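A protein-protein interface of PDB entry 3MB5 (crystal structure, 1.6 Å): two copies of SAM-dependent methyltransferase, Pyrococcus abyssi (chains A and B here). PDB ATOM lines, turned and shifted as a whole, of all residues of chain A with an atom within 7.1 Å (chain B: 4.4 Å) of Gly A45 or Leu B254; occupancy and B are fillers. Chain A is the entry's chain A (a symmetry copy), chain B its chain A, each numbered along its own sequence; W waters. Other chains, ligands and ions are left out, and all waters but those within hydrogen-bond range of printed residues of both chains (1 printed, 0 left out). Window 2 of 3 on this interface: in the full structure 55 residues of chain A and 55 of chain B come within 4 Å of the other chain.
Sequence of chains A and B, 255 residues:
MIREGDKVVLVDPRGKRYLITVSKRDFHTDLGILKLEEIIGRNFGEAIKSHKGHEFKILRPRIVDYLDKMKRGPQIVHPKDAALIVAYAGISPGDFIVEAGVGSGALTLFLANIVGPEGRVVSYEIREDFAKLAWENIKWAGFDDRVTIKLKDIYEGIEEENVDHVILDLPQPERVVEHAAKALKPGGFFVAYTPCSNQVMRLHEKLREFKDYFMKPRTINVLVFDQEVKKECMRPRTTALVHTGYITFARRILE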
ATOM      1  N   ILE A   2      -8.132  -0.135 -26.107  1.00  0.00           N
ATOM      2  CA  ILE A   2      -7.808   0.335 -27.445  1.00  0.00           C
ATOM      3  C   ILE A   2      -7.418  -0.829 -28.360  1.00  0.00           C
ATOM      4  O   ILE A   2      -6.691  -1.737 -27.941  1.00  0.00           O
ATOM      5  CB  ILE A   2      -6.674   1.374 -27.369  1.00  0.00           C
ATOM      6  CG1 ILE A   2      -7.089   2.504 -26.421  1.00  0.00           C
ATOM      7  CG2 ILE A   2      -6.301   1.905 -28.758  1.00  0.00           C
ATOM      8  CD1 ILE A   2      -5.926   3.316 -25.884  1.00  0.00           C
ATOM      9  N   ASN A  43      -5.685   1.258 -22.049  1.00  0.00           N
ATOM     10  CA  ASN A  43      -6.853   2.097 -21.833  1.00  0.00           C
ATOM     11  C   ASN A  43      -6.447   3.562 -21.861  1.00  0.00           C
ATOM     12  O   ASN A  43      -5.309   3.907 -21.535  1.00  0.00           O
ATOM     13  CB  ASN A  43      -7.480   1.788 -20.481  1.00  0.00           C
ATOM     14  CG  ASN A  43      -8.281   0.519 -20.496  1.00  0.00           C
ATOM     15  OD1 ASN A  43      -9.170   0.341 -21.330  1.00  0.00           O
ATOM     16  ND2 ASN A  43      -7.976  -0.375 -19.567  1.00  0.00           N
ATOM     17  N   PHE A  44      -7.392   4.419 -22.232  1.00  0.00           N
ATOM     18  CA  PHE A  44      -7.137   5.863 -22.183  1.00  0.00           C
ATOM     19  C   PHE A  44      -6.740   6.298 -20.801  1.00  0.00           C
ATOM     20  O   PHE A  44      -7.262   5.798 -19.797  1.00  0.00           O
ATOM     21  CB  PHE A  44      -8.365   6.619 -22.682  1.00  0.00           C
ATOM     22  CG  PHE A  44      -8.662   6.355 -24.121  1.00  0.00           C
ATOM     23  CD1 PHE A  44      -7.790   6.794 -25.112  1.00  0.00           C
ATOM     24  CD2 PHE A  44      -9.783   5.619 -24.497  1.00  0.00           C
ATOM     25  CE1 PHE A  44      -8.050   6.543 -26.447  1.00  0.00           C
ATOM     26  CE2 PHE A  44     -10.038   5.360 -25.838  1.00  0.00           C
ATOM     27  CZ  PHE A  44      -9.173   5.819 -26.810  1.00  0.00           C
ATOM     28  N   GLY A  45      -5.802   7.239 -20.743  1.00  0.00           N
ATOM     29  CA  GLY A  45      -5.219   7.653 -19.475  1.00  0.00           C
ATOM     30  C   GLY A  45      -3.864   7.031 -19.190  1.00  0.00           C
ATOM     31  O   GLY A  45      -3.065   7.573 -18.412  1.00  0.00           O
ATOM     32  N   GLU A  46      -3.580   5.900 -19.835  1.00  0.00           N
ATOM     33  CA  GLU A  46      -2.251   5.270 -19.702  1.00  0.00           C
ATOM     34  C   GLU A  46      -1.206   5.961 -20.596  1.00  0.00           C
ATOM     35  O   GLU A  46      -1.496   6.976 -21.261  1.00  0.00           O
ATOM     36  CB  GLU A  46      -2.346   3.758 -19.976  1.00  0.00           C
ATOM     37  CG  GLU A  46      -3.125   3.039 -18.883  1.00  0.00           C
ATOM     38  CD  GLU A  46      -3.532   1.601 -19.234  1.00  0.00           C
ATOM     39  OE1 GLU A  46      -3.097   1.066 -20.271  1.00  0.00           O
ATOM     40  OE2 GLU A  46      -4.297   1.006 -18.445  1.00  0.00           O
ATOM     41  N   ALA A  47       0.015   5.439 -20.607  1.00  0.00           N
ATOM     42  CA  ALA A  47       1.082   6.081 -21.349  1.00  0.00           C
ATOM     43  C   ALA A  47       2.029   5.053 -21.964  1.00  0.00           C
ATOM     44  O   ALA A  47       2.034   3.888 -21.559  1.00  0.00           O
ATOM     45  CB  ALA A  47       1.847   7.056 -20.443  1.00  0.00           C
ATOM     46  N   GLU A  55       7.760  10.180 -22.094  1.00  0.00           N
ATOM     47  CA  GLU A  55       6.428   9.614 -21.912  1.00  0.00           C
ATOM     48  C   GLU A  55       5.412  10.303 -22.820  1.00  0.00           C
ATOM     49  O   GLU A  55       5.417  11.535 -22.928  1.00  0.00           O
ATOM     50  CB  GLU A  55       5.991   9.764 -20.457  1.00  0.00           C
ATOM     51  CG  GLU A  55       4.774   8.945 -20.163  1.00  0.00           C
ATOM     52  CD  GLU A  55       4.389   8.986 -18.707  1.00  0.00           C
ATOM     53  OE1 GLU A  55       3.917  10.040 -18.259  1.00  0.00           O
ATOM     54  OE2 GLU A  55       4.556   7.961 -18.022  1.00  0.00           O
ATOM     55  N   LYS A  57       1.291  10.367 -23.258  1.00  0.00           N
ATOM     56  CA  LYS A  57       0.057  10.018 -22.561  1.00  0.00           C
ATOM     57  C   LYS A  57      -1.046   9.812 -23.587  1.00  0.00           C
ATOM     58  O   LYS A  57      -1.068  10.502 -24.594  1.00  0.00           O
ATOM     59  CB  LYS A  57      -0.295  11.131 -21.562  1.00  0.00           C
ATOM     60  CG  LYS A  57       0.781  11.231 -20.462  1.00  0.00           C
ATOM     61  CD  LYS A  57       0.619  12.444 -19.531  1.00  0.00           C
ATOM     62  CE  LYS A  57       1.630  12.452 -18.384  1.00  0.00           C
ATOM     63  NZ  LYS A  57       3.007  12.777 -18.863  1.00  0.00           N
ATOM     64  N   ILE A  58      -1.919   8.835 -23.349  1.00  0.00           N
ATOM     65  CA  ILE A  58      -2.919   8.414 -24.347  1.00  0.00           C
ATOM     66  C   ILE A  58      -4.316   8.942 -24.016  1.00  0.00           C
ATOM     67  O   ILE A  58      -4.844   8.670 -22.933  1.00  0.00           O
ATOM     68  CB  ILE A  58      -2.971   6.858 -24.460  1.00  0.00           C
ATOM     69  CG1 ILE A  58      -1.571   6.285 -24.679  1.00  0.00           C
ATOM     70  CG2 ILE A  58      -3.913   6.418 -25.592  1.00  0.00           C
ATOM     71  CD1 ILE A  58      -1.473   4.790 -24.231  1.00  0.00           C
ATOM     72  N   LEU A  59      -4.900   9.723 -24.936  1.00  0.00           N
ATOM     73  CA  LEU A  59      -6.227  10.318 -24.734  1.00  0.00           C
ATOM     74  C   LEU A  59      -7.153   9.948 -25.895  1.00  0.00           C
ATOM     75  O   LEU A  59      -6.690   9.712 -27.032  1.00  0.00           O
ATOM     76  CB  LEU A  59      -6.122  11.860 -24.696  1.00  0.00           C
ATOM     77  CG  LEU A  59      -5.383  12.530 -23.533  1.00  0.00           C
ATOM     78  CD1 LEU A  59      -5.484  14.056 -23.719  1.00  0.00           C
ATOM     79  CD2 LEU A  59      -5.989  12.112 -22.208  1.00  0.00           C
ATOM     80  N   ARG A  60      -8.460   9.932 -25.620  1.00  0.00           N
ATOM     81  CA  ARG A  60      -9.447   9.683 -26.675  1.00  0.00           C
ATOM     82  C   ARG A  60      -9.604  10.931 -27.532  1.00  0.00           C
ATOM     83  O   ARG A  60      -9.742  12.038 -26.992  1.00  0.00           O
ATOM     84  CB  ARG A  60     -10.793   9.253 -26.088  1.00  0.00           C
ATOM     85  CG  ARG A  60     -11.755   8.744 -27.161  1.00  0.00           C
ATOM     86  CD  ARG A  60     -13.133   8.501 -26.584  1.00  0.00           C
ATOM     87  NE  ARG A  60     -13.137   7.467 -25.551  1.00  0.00           N
ATOM     88  CZ  ARG A  60     -13.339   6.171 -25.792  1.00  0.00           C
ATOM     89  NH1 ARG A  60     -13.533   5.747 -27.029  1.00  0.00           N
ATOM     90  NH2 ARG A  60     -13.334   5.302 -24.794  1.00  0.00           N
ATOM     91  N   PRO B 186      -9.909  11.195 -18.314  1.00  0.00           N
ATOM     92  CA  PRO B 186      -8.718  11.667 -19.038  1.00  0.00           C
ATOM     93  C   PRO B 186      -9.135  12.447 -20.276  1.00  0.00           C
ATOM     94  O   PRO B 186      -9.957  11.972 -21.052  1.00  0.00           O
ATOM     95  CB  PRO B 186      -7.999  10.369 -19.453  1.00  0.00           C
ATOM     96  CG  PRO B 186      -8.468   9.342 -18.425  1.00  0.00           C
ATOM     97  CD  PRO B 186      -9.865   9.743 -18.007  1.00  0.00           C
ATOM     98  N   ARG B 252      -7.793  17.738 -18.508  1.00  0.00           N
ATOM     99  CA  ARG B 252      -7.320  16.743 -17.525  1.00  0.00           C
ATOM    100  C   ARG B 252      -6.370  15.747 -18.198  1.00  0.00           C
ATOM    101  O   ARG B 252      -6.656  15.225 -19.289  1.00  0.00           O
ATOM    102  CB  ARG B 252      -8.532  16.012 -16.957  1.00  0.00           C
ATOM    103  CG  ARG B 252      -8.210  14.872 -15.944  1.00  0.00           C
ATOM    104  CD  ARG B 252      -7.777  15.457 -14.631  1.00  0.00           C
ATOM    105  NE  ARG B 252      -7.712  14.403 -13.611  1.00  0.00           N
ATOM    106  CZ  ARG B 252      -6.597  13.791 -13.220  1.00  0.00           C
ATOM    107  NH1 ARG B 252      -6.672  12.844 -12.290  1.00  0.00           N
ATOM    108  NH2 ARG B 252      -5.421  14.121 -13.731  1.00  0.00           N
ATOM    109  N   ILE B 253      -5.228  15.507 -17.552  1.00  0.00           N
ATOM    110  CA  ILE B 253      -4.273  14.508 -18.045  1.00  0.00           C
ATOM    111  C   ILE B 253      -3.633  13.819 -16.833  1.00  0.00           C
ATOM    112  O   ILE B 253      -3.311  14.479 -15.856  1.00  0.00           O
ATOM    113  CB  ILE B 253      -3.237  15.134 -19.005  1.00  0.00           C
ATOM    114  CG1 ILE B 253      -2.504  14.062 -19.787  1.00  0.00           C
ATOM    115  CG2 ILE B 253      -2.260  16.088 -18.272  1.00  0.00           C
ATOM    116  CD1 ILE B 253      -2.153  14.507 -21.184  1.00  0.00           C
ATOM    117  N   LEU B 254      -3.461  12.501 -16.909  1.00  0.00           N
ATOM    118  CA  LEU B 254      -3.044  11.711 -15.738  1.00  0.00           C
ATOM    119  C   LEU B 254      -1.528  11.636 -15.608  1.00  0.00           C
ATOM    120  O   LEU B 254      -0.842  11.253 -16.559  1.00  0.00           O
ATOM    121  CB  LEU B 254      -3.630  10.282 -15.786  1.00  0.00           C
ATOM    122  CG  LEU B 254      -5.147  10.061 -15.769  1.00  0.00           C
ATOM    123  CD1 LEU B 254      -5.794  10.831 -16.889  1.00  0.00           C
ATOM    124  CD2 LEU B 254      -5.514   8.562 -15.867  1.00  0.00           C
ATOM    125  N   GLU B 255      -1.044  12.017 -14.422  1.00  0.00           N
ATOM    126  CA  GLU B 255       0.346  11.831 -13.950  1.00  0.00           C
ATOM    127  C   GLU B 255       1.376  12.787 -14.548  1.00  0.00           C
ATOM    128  O   GLU B 255       2.134  13.429 -13.807  1.00  0.00           O
ATOM    129  CB  GLU B 255       0.806  10.368 -14.066  1.00  0.00           C
ATOM    130  CG  GLU B 255       0.172   9.424 -13.041  1.00  0.00           C
ATOM    131  CD  GLU B 255       0.979   9.289 -11.740  1.00  0.00           C
ATOM    132  OE1 GLU B 255       2.166   9.696 -11.699  1.00  0.00           O
ATOM    133  OE2 GLU B 255       0.421   8.755 -10.752  1.00  0.00           O
HETATM  134  O   HOH W   1      -9.528   9.904 -22.932  1.00  0.00           O
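The backbone NH (N) of Gly A45 is in hydrogen-bond range of the backbone carbonyl oxygen (O) of Ile A58, at 2.8 Å. The side-chain carboxylate (OE1) of Glu A55 lies within salt-bridge range of the side-chain amino group (NZ) of Lys A57 (2.9 Å).
Pro B186 touches Phe A44 (CG to O, 3.99 Å). Gly A45 touches Pro B186. Gly A45 touches Leu B254. Lys A57 touches Ile B253. Lys A57 touches Leu B254. C of Glu B255 touches CE of Lys A57, at 3.9 Å. CD2 of Leu A59 touches C of Pro B186, at 3.7 Å.
Of the printed residues of chain B, Lys A57 touches Ile B253, Leu B254 and Glu B255. Arg A60 touches none of the printed residues of chain B. Of the printed residues of chain A, Pro B186 touches Phe A44, Gly A45 and Leu A59. Printed residues of chain A within 4 Å of Ile B253: Lys A57 (3.5 Å). Of chain A, only Gly A45 and Lys A57 come within 4 Å of Leu B254. Of the printed residues of chain A, Glu B255 touches Lys A57.
Of the 11 printed residues of chain A, 4 touch a printed residue of chain B. Hydrophobic or aromatic side chains of chain A that line the printed part of chain B: Leu A59. Of the 5 printed residues of chain B, 4 touch a printed residue of chain A. Hydrophobic or aromatic side chains of chain B that line the printed part of chain A: Pro B186, Ile B253 and Leu B254. Along chain B the printed residues that touch a printed residue of chain A span positions 186 to 255.
No position is printed for both chains.
Water W1 bridges O of Pro B186 (2.8 Å) and N of Arg A60 (2.9 Å).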
